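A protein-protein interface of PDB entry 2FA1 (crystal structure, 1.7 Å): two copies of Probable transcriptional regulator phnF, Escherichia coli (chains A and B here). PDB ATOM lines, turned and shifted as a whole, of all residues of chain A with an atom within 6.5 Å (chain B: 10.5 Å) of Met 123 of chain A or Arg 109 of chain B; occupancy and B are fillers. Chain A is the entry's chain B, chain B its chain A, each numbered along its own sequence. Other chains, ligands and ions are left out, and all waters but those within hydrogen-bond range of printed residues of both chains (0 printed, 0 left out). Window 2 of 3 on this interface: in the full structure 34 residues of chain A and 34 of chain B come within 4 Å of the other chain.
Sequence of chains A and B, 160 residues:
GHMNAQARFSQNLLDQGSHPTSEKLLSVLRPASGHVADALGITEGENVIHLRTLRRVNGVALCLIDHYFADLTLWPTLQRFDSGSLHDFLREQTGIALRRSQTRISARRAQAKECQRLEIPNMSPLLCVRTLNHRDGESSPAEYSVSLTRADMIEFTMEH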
ATOM      1  N   ARG A 108     -11.102   2.805  -6.723  1.00  0.00           N
ATOM      2  CA  ARG A 108     -11.922   3.622  -7.654  1.00  0.00           C
ATOM      3  C   ARG A 108     -11.173   4.839  -8.107  1.00  0.00           C
ATOM      4  O   ARG A 108     -10.140   5.151  -7.569  1.00  0.00           O
ATOM      5  CB  ARG A 108     -13.206   4.055  -6.976  1.00  0.00           C
ATOM      6  CG  ARG A 108     -12.999   4.802  -5.672  1.00  0.00           C
ATOM      7  CD  ARG A 108     -13.713   4.118  -4.482  1.00  0.00           C
ATOM      8  NE  ARG A 108     -14.141   5.031  -3.387  1.00  0.00           N
ATOM      9  CZ  ARG A 108     -14.342   6.351  -3.496  1.00  0.00           C
ATOM     10  NH1 ARG A 108     -14.207   6.997  -4.654  1.00  0.00           N
ATOM     11  NH2 ARG A 108     -14.679   7.046  -2.421  1.00  0.00           N
ATOM     12  N   ARG A 109     -11.732   5.506  -9.121  1.00  0.00           N
ATOM     13  CA  ARG A 109     -11.140   6.753  -9.601  1.00  0.00           C
ATOM     14  C   ARG A 109     -11.582   7.859  -8.642  1.00  0.00           C
ATOM     15  O   ARG A 109     -12.699   7.818  -8.148  1.00  0.00           O
ATOM     16  CB  ARG A 109     -11.518   6.973 -11.071  1.00  0.00           C
ATOM     17  CG  ARG A 109     -10.566   6.201 -11.965  1.00  0.00           C
ATOM     18  CD  ARG A 109     -10.748   6.457 -13.460  1.00  0.00           C
ATOM     19  NE  ARG A 109     -11.912   5.727 -13.987  1.00  0.00           N
ATOM     20  CZ  ARG A 109     -11.887   4.918 -15.050  1.00  0.00           C
ATOM     21  NH1 ARG A 109     -10.759   4.749 -15.739  1.00  0.00           N
ATOM     22  NH2 ARG A 109     -13.000   4.302 -15.453  1.00  0.00           N
ATOM     23  N   ALA A 110     -10.656   8.767  -8.283  1.00  0.00           N
ATOM     24  CA  ALA A 110     -10.964   9.877  -7.393  1.00  0.00           C
ATOM     25  C   ALA A 110     -11.940  10.833  -8.073  1.00  0.00           C
ATOM     26  O   ALA A 110     -11.727  11.251  -9.253  1.00  0.00           O
ATOM     27  CB  ALA A 110      -9.688  10.641  -6.991  1.00  0.00           C
ATOM     28  N   GLN A 111     -13.012  11.122  -7.342  1.00  0.00           N
ATOM     29  CA  GLN A 111     -13.972  12.114  -7.780  1.00  0.00           C
ATOM     30  C   GLN A 111     -14.145  13.272  -6.762  1.00  0.00           C
ATOM     31  O   GLN A 111     -14.105  13.080  -5.515  1.00  0.00           O
ATOM     32  CB  GLN A 111     -15.314  11.433  -8.083  1.00  0.00           C
ATOM     33  CG  GLN A 111     -16.034  11.959  -9.349  1.00  0.00           C
ATOM     34  CD  GLN A 111     -16.901  10.879 -10.022  1.00  0.00           C
ATOM     35  OE1 GLN A 111     -16.789  10.636 -11.235  1.00  0.00           O
ATOM     36  NE2 GLN A 111     -17.766  10.223  -9.228  1.00  0.00           N
ATOM     37  N   ALA A 112     -14.344  14.472  -7.320  1.00  0.00           N
ATOM     38  CA  ALA A 112     -14.980  15.566  -6.584  1.00  0.00           C
ATOM     39  C   ALA A 112     -14.123  16.088  -5.454  1.00  0.00           C
ATOM     40  O   ALA A 112     -12.958  16.509  -5.666  1.00  0.00           O
ATOM     41  CB  ALA A 112     -16.407  15.130  -6.045  1.00  0.00           C
ATOM     42  N   CYS A 115     -10.444  14.389  -4.786  1.00  0.00           N
ATOM     43  CA  CYS A 115      -9.287  14.966  -5.486  1.00  0.00           C
ATOM     44  C   CYS A 115      -8.776  16.162  -4.744  1.00  0.00           C
ATOM     45  O   CYS A 115      -7.578  16.376  -4.650  1.00  0.00           O
ATOM     46  CB  CYS A 115      -9.633  15.487  -6.879  1.00  0.00           C
ATOM     47  SG  CYS A 115     -10.155  14.244  -7.893  1.00  0.00           S
ATOM     48  N   ILE A 120      -4.941  15.660  -5.588  1.00  0.00           N
ATOM     49  CA  ILE A 120      -4.594  14.810  -6.760  1.00  0.00           C
ATOM     50  C   ILE A 120      -5.525  15.112  -7.913  1.00  0.00           C
ATOM     51  O   ILE A 120      -6.642  15.638  -7.688  1.00  0.00           O
ATOM     52  CB  ILE A 120      -4.668  13.288  -6.386  1.00  0.00           C
ATOM     53  CG1 ILE A 120      -6.113  12.946  -5.878  1.00  0.00           C
ATOM     54  CG2 ILE A 120      -3.573  12.979  -5.332  1.00  0.00           C
ATOM     55  CD1 ILE A 120      -6.312  11.554  -5.547  1.00  0.00           C
ATOM     56  N   PRO A 121      -5.054  14.844  -9.165  1.00  0.00           N
ATOM     57  CA  PRO A 121      -5.819  15.184 -10.345  1.00  0.00           C
ATOM     58  C   PRO A 121      -7.070  14.339 -10.386  1.00  0.00           C
ATOM     59  O   PRO A 121      -7.106  13.219  -9.823  1.00  0.00           O
ATOM     60  CB  PRO A 121      -4.894  14.822 -11.507  1.00  0.00           C
ATOM     61  CG  PRO A 121      -3.445  14.756 -10.869  1.00  0.00           C
ATOM     62  CD  PRO A 121      -3.755  14.222  -9.480  1.00  0.00           C
ATOM     63  N   ASN A 122      -8.096  14.877 -11.031  1.00  0.00           N
ATOM     64  CA  ASN A 122      -9.298  14.122 -11.268  1.00  0.00           C
ATOM     65  C   ASN A 122      -9.015  12.721 -11.876  1.00  0.00           C
ATOM     66  O   ASN A 122      -8.124  12.580 -12.734  1.00  0.00           O
ATOM     67  CB  ASN A 122     -10.238  14.896 -12.181  1.00  0.00           C
ATOM     68  CG  ASN A 122     -11.615  14.286 -12.173  1.00  0.00           C
ATOM     69  OD1 ASN A 122     -12.419  14.527 -11.253  1.00  0.00           O
ATOM     70  ND2 ASN A 122     -11.870  13.429 -13.145  1.00  0.00           N
ATOM     71  N   MET A 123      -9.773  11.713 -11.413  1.00  0.00           N
ATOM     72  CA  MET A 123      -9.667  10.293 -11.842  1.00  0.00           C
ATOM     73  C   MET A 123      -8.365   9.531 -11.452  1.00  0.00           C
ATOM     74  O   MET A 123      -8.140   8.408 -11.932  1.00  0.00           O
ATOM     75  CB  MET A 123      -9.977  10.105 -13.377  1.00  0.00           C
ATOM     76  CG  MET A 123     -11.438  10.477 -13.891  1.00  0.00           C
ATOM     77  SD  MET A 123     -12.915   9.582 -13.185  1.00  0.00           S
ATOM     78  CE  MET A 123     -13.557  10.721 -11.950  1.00  0.00           C
ATOM     79  N   SER A 124      -7.521  10.095 -10.578  1.00  0.00           N
ATOM     80  CA  SER A 124      -6.290   9.400 -10.139  1.00  0.00           C
ATOM     81  C   SER A 124      -6.829   8.190  -9.342  1.00  0.00           C
ATOM     82  O   SER A 124      -7.830   8.362  -8.645  1.00  0.00           O
ATOM     83  CB  SER A 124      -5.498  10.363  -9.222  1.00  0.00           C
ATOM     84  OG  SER A 124      -4.125  10.034  -9.082  1.00  0.00           O
ATOM     85  N   PRO A 125      -6.222   6.984  -9.467  1.00  0.00           N
ATOM     86  CA  PRO A 125      -6.811   5.841  -8.726  1.00  0.00           C
ATOM     87  C   PRO A 125      -6.622   5.964  -7.194  1.00  0.00           C
ATOM     88  O   PRO A 125      -5.515   6.377  -6.742  1.00  0.00           O
ATOM     89  CB  PRO A 125      -6.074   4.627  -9.318  1.00  0.00           C
ATOM     90  CG  PRO A 125      -4.744   5.184  -9.718  1.00  0.00           C
ATOM     91  CD  PRO A 125      -5.097   6.547 -10.308  1.00  0.00           C
ATOM     92  N   LEU A 126      -7.650   5.534  -6.428  1.00  0.00           N
ATOM     93  CA  LEU A 126      -7.549   5.507  -4.962  1.00  0.00           C
ATOM     94  C   LEU A 126      -7.772   4.099  -4.530  1.00  0.00           C
ATOM     95  O   LEU A 126      -8.549   3.350  -5.211  1.00  0.00           O
ATOM     96  CB  LEU A 126      -8.586   6.400  -4.304  1.00  0.00           C
ATOM     97  CG  LEU A 126      -8.460   7.902  -4.589  1.00  0.00           C
ATOM     98  CD1 LEU A 126      -9.516   8.681  -3.861  1.00  0.00           C
ATOM     99  CD2 LEU A 126      -7.053   8.334  -4.262  1.00  0.00           C
ATOM    100  N   SER B 106      -2.319  -3.776  -4.197  1.00  0.00           N
ATOM    101  CA  SER B 106      -2.152  -2.449  -4.802  1.00  0.00           C
ATOM    102  C   SER B 106      -3.266  -2.155  -5.796  1.00  0.00           C
ATOM    103  O   SER B 106      -4.048  -3.013  -6.126  1.00  0.00           O
ATOM    104  CB  SER B 106      -0.836  -2.435  -5.553  1.00  0.00           C
ATOM    105  OG  SER B 106      -0.775  -3.443  -6.549  1.00  0.00           O
ATOM    106  N   ALA B 107      -3.223  -0.944  -6.363  1.00  0.00           N
ATOM    107  CA  ALA B 107      -4.239  -0.631  -7.426  1.00  0.00           C
ATOM    108  C   ALA B 107      -3.492   0.093  -8.492  1.00  0.00           C
ATOM    109  O   ALA B 107      -2.613   0.922  -8.226  1.00  0.00           O
ATOM    110  CB  ALA B 107      -5.401   0.193  -6.952  1.00  0.00           C
ATOM    111  N   ARG B 108      -3.867  -0.204  -9.705  1.00  0.00           N
ATOM    112  CA  ARG B 108      -3.265   0.529 -10.822  1.00  0.00           C
ATOM    113  C   ARG B 108      -4.144   0.569 -12.026  1.00  0.00           C
ATOM    114  O   ARG B 108      -5.260   0.063 -12.008  1.00  0.00           O
ATOM    115  CB  ARG B 108      -1.903  -0.043 -11.100  1.00  0.00           C
ATOM    116  CG  ARG B 108      -1.951  -1.492 -11.597  1.00  0.00           C
ATOM    117  CD  ARG B 108      -0.604  -1.723 -12.280  1.00  0.00           C
ATOM    118  NE  ARG B 108      -0.422  -3.094 -12.798  1.00  0.00           N
ATOM    119  CZ  ARG B 108      -0.065  -4.143 -12.063  1.00  0.00           C
ATOM    120  NH1 ARG B 108       0.129  -5.343 -12.615  1.00  0.00           N
ATOM    121  NH2 ARG B 108       0.099  -4.000 -10.772  1.00  0.00           N
ATOM    122  N   ARG B 109      -3.705   1.326 -13.027  1.00  0.00           N
ATOM    123  CA  ARG B 109      -4.560   1.574 -14.195  1.00  0.00           C
ATOM    124  C   ARG B 109      -4.060   0.638 -15.258  1.00  0.00           C
ATOM    125  O   ARG B 109      -2.871   0.616 -15.533  1.00  0.00           O
ATOM    126  CB  ARG B 109      -4.544   3.080 -14.603  1.00  0.00           C
ATOM    127  CG  ARG B 109      -5.572   3.900 -13.738  1.00  0.00           C
ATOM    128  CD  ARG B 109      -5.698   5.354 -14.113  1.00  0.00           C
ATOM    129  NE  ARG B 109      -4.515   6.108 -13.731  1.00  0.00           N
ATOM    130  CZ  ARG B 109      -4.366   7.434 -13.889  1.00  0.00           C
ATOM    131  NH1 ARG B 109      -5.335   8.154 -14.435  1.00  0.00           N
ATOM    132  NH2 ARG B 109      -3.247   8.048 -13.478  1.00  0.00           N
ATOM    133  N   ALA B 110      -4.959  -0.168 -15.842  1.00  0.00           N
ATOM    134  CA  ALA B 110      -4.557  -1.245 -16.757  1.00  0.00           C
ATOM    135  C   ALA B 110      -3.988  -0.697 -18.040  1.00  0.00           C
ATOM    136  O   ALA B 110      -4.511   0.258 -18.573  1.00  0.00           O
ATOM    137  CB  ALA B 110      -5.767  -2.091 -17.130  1.00  0.00           C
ATOM    138  N   GLN B 111      -2.912  -1.351 -18.490  1.00  0.00           N
ATOM    139  CA  GLN B 111      -2.337  -1.093 -19.792  1.00  0.00           C
ATOM    140  C   GLN B 111      -1.856  -2.371 -20.503  1.00  0.00           C
ATOM    141  O   GLN B 111      -1.575  -3.449 -19.867  1.00  0.00           O
ATOM    142  CB  GLN B 111      -1.247  -0.006 -19.702  1.00  0.00           C
ATOM    143  CG  GLN B 111      -1.797   1.401 -19.323  1.00  0.00           C
ATOM    144  CD  GLN B 111      -0.661   2.421 -19.332  1.00  0.00           C
ATOM    145  OE1 GLN B 111       0.139   2.443 -18.417  1.00  0.00           O
ATOM    146  NE2 GLN B 111      -0.608   3.262 -20.358  1.00  0.00           N
ATOM    147  N   ALA B 112      -1.804  -2.253 -21.834  1.00  0.00           N
ATOM    148  CA  ALA B 112      -1.152  -3.269 -22.685  1.00  0.00           C
ATOM    149  C   ALA B 112      -1.720  -4.665 -22.422  1.00  0.00           C
ATOM    150  O   ALA B 112      -2.931  -4.912 -22.611  1.00  0.00           O
ATOM    151  CB  ALA B 112       0.396  -3.253 -22.435  1.00  0.00           C
ATOM    152  N   LYS B 113      -0.877  -5.587 -21.981  1.00  0.00           N
ATOM    153  CA  LYS B 113      -1.361  -6.970 -21.939  1.00  0.00           C
ATOM    154  C   LYS B 113      -2.391  -7.187 -20.832  1.00  0.00           C
ATOM    155  O   LYS B 113      -3.222  -8.076 -20.996  1.00  0.00           O
ATOM    156  CB  LYS B 113      -0.239  -7.987 -21.777  1.00  0.00           C
ATOM    157  CG  LYS B 113       0.375  -8.162 -20.357  1.00  0.00           C
ATOM    158  CD  LYS B 113       0.835  -6.883 -19.563  1.00  0.00           C
ATOM    159  CE  LYS B 113       2.212  -6.321 -20.004  1.00  0.00           C
ATOM    160  NZ  LYS B 113       2.306  -6.091 -21.482  1.00  0.00           N
ATOM    161  N   GLU B 114      -2.400  -6.342 -19.795  1.00  0.00           N
ATOM    162  CA  GLU B 114      -3.477  -6.383 -18.802  1.00  0.00           C
ATOM    163  C   GLU B 114      -4.818  -6.057 -19.441  1.00  0.00           C
ATOM    164  O   GLU B 114      -5.831  -6.741 -19.150  1.00  0.00           O
ATOM    165  CB  GLU B 114      -3.180  -5.396 -17.657  1.00  0.00           C
ATOM    166  CG  GLU B 114      -1.944  -5.723 -16.858  1.00  0.00           C
ATOM    167  CD  GLU B 114      -1.449  -4.511 -16.079  1.00  0.00           C
ATOM    168  OE1 GLU B 114      -1.887  -3.326 -16.331  1.00  0.00           O
ATOM    169  OE2 GLU B 114      -0.575  -4.758 -15.236  1.00  0.00           O
ATOM    170  N   CYS B 115      -4.864  -5.071 -20.346  1.00  0.00           N
ATOM    171  CA  CYS B 115      -6.127  -4.682 -21.007  1.00  0.00           C
ATOM    172  C   CYS B 115      -6.523  -5.809 -21.954  1.00  0.00           C
ATOM    173  O   CYS B 115      -7.712  -6.057 -22.153  1.00  0.00           O
ATOM    174  CB  CYS B 115      -6.040  -3.421 -21.843  1.00  0.00           C
ATOM    175  SG  CYS B 115      -5.716  -1.944 -20.935  1.00  0.00           S
ATOM    176  N   GLN B 116      -5.520  -6.511 -22.513  1.00  0.00           N
ATOM    177  CA  GLN B 116      -5.838  -7.588 -23.465  1.00  0.00           C
ATOM    178  C   GLN B 116      -6.424  -8.775 -22.738  1.00  0.00           C
ATOM    179  O   GLN B 116      -7.528  -9.271 -23.133  1.00  0.00           O
ATOM    180  CB  GLN B 116      -4.627  -7.966 -24.373  1.00  0.00           C
ATOM    181  CG  GLN B 116      -4.916  -9.183 -25.307  1.00  0.00           C
ATOM    182  CD  GLN B 116      -3.704  -9.627 -26.176  1.00  0.00           C
ATOM    183  OE1 GLN B 116      -3.776 -10.623 -26.916  1.00  0.00           O
ATOM    184  NE2 GLN B 116      -2.605  -8.909 -26.076  1.00  0.00           N
ATOM    185  N   LEU B 118      -7.784  -8.930 -19.625  1.00  0.00           N
ATOM    186  CA  LEU B 118      -9.018  -8.685 -18.892  1.00  0.00           C
ATOM    187  C   LEU B 118     -10.033  -8.023 -19.779  1.00  0.00           C
ATOM    188  O   LEU B 118     -11.151  -7.762 -19.289  1.00  0.00           O
ATOM    189  CB  LEU B 118      -8.824  -7.821 -17.639  1.00  0.00           C
ATOM    190  CG  LEU B 118      -8.325  -8.577 -16.402  1.00  0.00           C
ATOM    191  CD1 LEU B 118      -8.033  -7.619 -15.311  1.00  0.00           C
ATOM    192  CD2 LEU B 118      -9.463  -9.449 -15.875  1.00  0.00           C
ATOM    193  N   ILE B 120     -10.409  -5.030 -21.227  1.00  0.00           N
ATOM    194  CA  ILE B 120     -10.889  -3.711 -20.706  1.00  0.00           C
ATOM    195  C   ILE B 120     -10.182  -2.583 -21.381  1.00  0.00           C
ATOM    196  O   ILE B 120      -9.147  -2.824 -21.927  1.00  0.00           O
ATOM    197  CB  ILE B 120     -10.686  -3.599 -19.198  1.00  0.00           C
ATOM    198  CG1 ILE B 120      -9.276  -4.029 -18.873  1.00  0.00           C
ATOM    199  CG2 ILE B 120     -11.789  -4.483 -18.474  1.00  0.00           C
ATOM    200  CD1 ILE B 120      -8.900  -3.964 -17.498  1.00  0.00           C
ATOM    201  N   PRO B 121     -10.727  -1.354 -21.323  1.00  0.00           N
ATOM    202  CA  PRO B 121     -10.109  -0.205 -21.932  1.00  0.00           C
ATOM    203  C   PRO B 121      -8.850   0.220 -21.236  1.00  0.00           C
ATOM    204  O   PRO B 121      -8.598  -0.078 -20.025  1.00  0.00           O
ATOM    205  CB  PRO B 121     -11.175   0.914 -21.799  1.00  0.00           C
ATOM    206  CG  PRO B 121     -12.172   0.468 -20.991  1.00  0.00           C
ATOM    207  CD  PRO B 121     -11.997  -1.008 -20.672  1.00  0.00           C
ATOM    208  N   ASN B 122      -8.035   0.908 -22.029  1.00  0.00           N
ATOM    209  CA  ASN B 122      -6.866   1.538 -21.533  1.00  0.00           C
ATOM    210  C   ASN B 122      -7.196   2.342 -20.259  1.00  0.00           C
ATOM    211  O   ASN B 122      -8.195   3.055 -20.191  1.00  0.00           O
ATOM    212  CB  ASN B 122      -6.312   2.418 -22.670  1.00  0.00           C
ATOM    213  CG  ASN B 122      -4.948   2.920 -22.358  1.00  0.00           C
ATOM    214  OD1 ASN B 122      -4.147   2.203 -21.746  1.00  0.00           O
ATOM    215  ND2 ASN B 122      -4.681   4.178 -22.705  1.00  0.00           N
ATOM    216  N   MET B 123      -6.347   2.185 -19.244  1.00  0.00           N
ATOM    217  CA  MET B 123      -6.378   2.949 -17.963  1.00  0.00           C
ATOM    218  C   MET B 123      -7.500   2.511 -16.974  1.00  0.00           C
ATOM    219  O   MET B 123      -7.700   3.100 -15.887  1.00  0.00           O
ATOM    220  CB  MET B 123      -6.400   4.475 -18.221  1.00  0.00           C
ATOM    221  CG  MET B 123      -5.165   4.872 -19.074  1.00  0.00           C
ATOM    222  SD  MET B 123      -3.575   4.561 -18.267  1.00  0.00           S
ATOM    223  CE  MET B 123      -3.719   5.749 -16.973  1.00  0.00           C
ATOM    224  N   SER B 124      -8.174   1.409 -17.307  1.00  0.00           N
ATOM    225  CA  SER B 124      -9.252   0.927 -16.419  1.00  0.00           C
ATOM    226  C   SER B 124      -8.645   0.518 -15.069  1.00  0.00           C
ATOM    227  O   SER B 124      -7.587  -0.163 -15.098  1.00  0.00           O
ATOM    228  CB  SER B 124      -9.890  -0.340 -17.000  1.00  0.00           C
ATOM    229  OG  SER B 124     -10.629  -0.011 -18.097  1.00  0.00           O
ATOM    230  N   PRO B 125      -9.129   1.063 -13.914  1.00  0.00           N
ATOM    231  CA  PRO B 125      -8.548   0.627 -12.610  1.00  0.00           C
ATOM    232  C   PRO B 125      -8.685  -0.868 -12.230  1.00  0.00           C
ATOM    233  O   PRO B 125      -9.817  -1.447 -12.255  1.00  0.00           O
ATOM    234  CB  PRO B 125      -9.283   1.513 -11.582  1.00  0.00           C
ATOM    235  CG  PRO B 125      -9.579   2.709 -12.329  1.00  0.00           C
ATOM    236  CD  PRO B 125     -10.054   2.187 -13.680  1.00  0.00           C
ATOM    237  N   LEU B 126      -7.544  -1.436 -11.803  1.00  0.00           N
ATOM    238  CA  LEU B 126      -7.472  -2.850 -11.390  1.00  0.00           C
ATOM    239  C   LEU B 126      -7.005  -2.941  -9.953  1.00  0.00           C
ATOM    240  O   LEU B 126      -6.163  -2.096  -9.562  1.00  0.00           O
ATOM    241  CB  LEU B 126      -6.486  -3.647 -12.220  1.00  0.00           C
ATOM    242  CG  LEU B 126      -6.534  -3.689 -13.731  1.00  0.00           C
ATOM    243  CD1 LEU B 126      -5.269  -4.430 -14.227  1.00  0.00           C
ATOM    244  CD2 LEU B 126      -7.817  -4.375 -14.068  1.00  0.00           C
ATOM    245  N   LEU B 127      -7.491  -3.942  -9.202  1.00  0.00           N
ATOM    246  CA  LEU B 127      -6.916  -4.275  -7.886  1.00  0.00           C
ATOM    247  C   LEU B 127      -5.933  -5.387  -8.168  1.00  0.00           C
ATOM    248  O   LEU B 127      -6.255  -6.356  -8.936  1.00  0.00           O
ATOM    249  CB  LEU B 127      -7.977  -4.805  -6.927  1.00  0.00           C
ATOM    250  CG  LEU B 127      -8.777  -3.727  -6.188  1.00  0.00           C
ATOM    251  CD1 LEU B 127     -10.224  -4.150  -5.678  1.00  0.00           C
ATOM    252  CD2 LEU B 127      -7.890  -3.148  -5.091  1.00  0.00           C
ATOM    253  N   CYS B 128      -4.719  -5.285  -7.613  1.00  0.00           N
ATOM    254  CA  CYS B 128      -3.738  -6.307  -7.819  1.00  0.00           C
ATOM    255  C   CYS B 128      -3.412  -6.927  -6.453  1.00  0.00           C
ATOM    256  O   CYS B 128      -3.043  -6.177  -5.523  1.00  0.00           O
ATOM    257  CB  CYS B 128      -2.523  -5.719  -8.441  1.00  0.00           C
ATOM    258  SG  CYS B 128      -1.057  -6.863  -8.509  1.00  0.00           S
ATOM    259  N   LEU B 148      -5.405 -10.091 -10.750  1.00  0.00           N
ATOM    260  CA  LEU B 148      -5.738  -8.745 -11.275  1.00  0.00           C
ATOM    261  C   LEU B 148      -7.250  -8.781 -11.484  1.00  0.00           C
ATOM    262  O   LEU B 148      -7.771  -9.688 -12.134  1.00  0.00           O
ATOM    263  CB  LEU B 148      -5.072  -8.484 -12.654  1.00  0.00           C
ATOM    264  CG  LEU B 148      -3.550  -8.517 -12.632  1.00  0.00           C
ATOM    265  CD1 LEU B 148      -3.210  -8.371 -14.085  1.00  0.00           C
ATOM    266  CD2 LEU B 148      -3.155  -7.358 -11.844  1.00  0.00           C
ATOM    267  N   THR B 149      -7.954  -7.895 -10.753  1.00  0.00           N
ATOM    268  CA  THR B 149      -9.401  -7.865 -10.745  1.00  0.00           C
ATOM    269  C   THR B 149      -9.940  -6.512 -11.092  1.00  0.00           C
ATOM    270  O   THR B 149      -9.534  -5.511 -10.559  1.00  0.00           O
ATOM    271  CB  THR B 149     -10.013  -8.122  -9.369  1.00  0.00           C
ATOM    272  OG1 THR B 149      -9.376  -7.274  -8.370  1.00  0.00           O
ATOM    273  CG2 THR B 149      -9.918  -9.553  -8.909  1.00  0.00           C
ATOM    274  N   ARG B 150     -10.950  -6.499 -11.948  1.00  0.00           N
ATOM    275  CA  ARG B 150     -11.537  -5.221 -12.349  1.00  0.00           C
ATOM    276  C   ARG B 150     -12.131  -4.558 -11.097  1.00  0.00           C
ATOM    277  O   ARG B 150     -13.018  -5.093 -10.405  1.00  0.00           O
ATOM    278  CB  ARG B 150     -12.736  -5.546 -13.324  1.00  0.00           C
ATOM    279  CG  ARG B 150     -12.240  -5.794 -14.783  1.00  0.00           C
ATOM    280  CD  ARG B 150     -13.527  -5.982 -15.665  1.00  0.00           C
ATOM    281  NE  ARG B 150     -14.358  -4.753 -15.708  1.00  0.00           N
ATOM    282  CZ  ARG B 150     -15.215  -4.486 -16.706  1.00  0.00           C
ATOM    283  NH1 ARG B 150     -15.282  -5.238 -17.813  1.00  0.00           N
ATOM    284  NH2 ARG B 150     -15.928  -3.333 -16.693  1.00  0.00           N
ATOM    285  N   ALA B 151     -11.594  -3.385 -10.771  1.00  0.00           N
ATOM    286  CA  ALA B 151     -12.039  -2.757  -9.562  1.00  0.00           C
ATOM    287  C   ALA B 151     -13.441  -2.179  -9.675  1.00  0.00           C
ATOM    288  O   ALA B 151     -14.065  -1.891  -8.637  1.00  0.00           O
ATOM    289  CB  ALA B 151     -11.048  -1.674  -9.185  1.00  0.00           C
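Printed residues of chain B within 4 Å of Arg 109 of chain A: Met 123 (3.5 Å) and Pro 125 (3.4 Å). Of chain B, only Arg 109 comes within 4 Å of Met 123 of chain A. Arg 109 of chain B touches just these residues of chain A: Met 123 (3.8 Å) and Pro 125 (3.5 Å). Of the printed residues of chain A, Met 123 of chain B touches Arg 109 (3.5 Å). Printed residues of chain A within 4 Å of Pro 125 of chain B: Arg 109. The nearest printed residue of chain B that does not touch Met 123 of chain A is Pro 125 of chain B (5.9 Å).
O of Met 123 of chain B is in hydrogen-bond range of NH1 of Arg 109 of chain A (3.5 Å).
Hydrophobic or aromatic side chains of chain A that line the printed part of chain B: Pro 125. Hydrophobic or aromatic side chains of chain B within 4 Å of the printed part of chain A: Pro 125. Among the printed residues, 4 pairs touch across the chains. Among the printed residues, no Asp or Glu carboxylate lies within 4 Å of a Lys or Arg side-chain nitrogen of the other chain.
Among the printed residues, pairs that only touch across the chains: Arg 109 of chain A with Pro 125 of chain B, Pro 125 of chain A with Arg 109 of chain B and Met 123 of chain A with Arg 109 of chain B.
O of Ala 110 of chain B is in hydrogen-bond range of N of Met 123 of chain B. The backbone NH (N) of Ala 151 of chain B sits at hydrogen-bond distance from the backbone carbonyl oxygen (O) of Pro 125 of chain B, at 3.0 Å. The backbone NH (N) of Met 123 of chain A lies within hydrogen-bond range of the backbone carbonyl oxygen (O) of Ala 110 of chain A, 2.9 Å away.
Arg 109 of chain A touches Met 123 of chain B, and with the chains exchanged Met 123 of chain A touches Arg 109 of chain B. Arg 109 of chain A touches Pro 125 of chain B, and with the chains exchanged Pro 125 of chain A touches Arg 109 of chain B. Positions printed for both chains: 108, 109, 110, 111, 112, 115, 120, 121, 122, 123, 124, 125 and 126. Of the 4 pairs that touch across the chains among the printed residues, 4 have their exchanged pair printed and touching as well.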
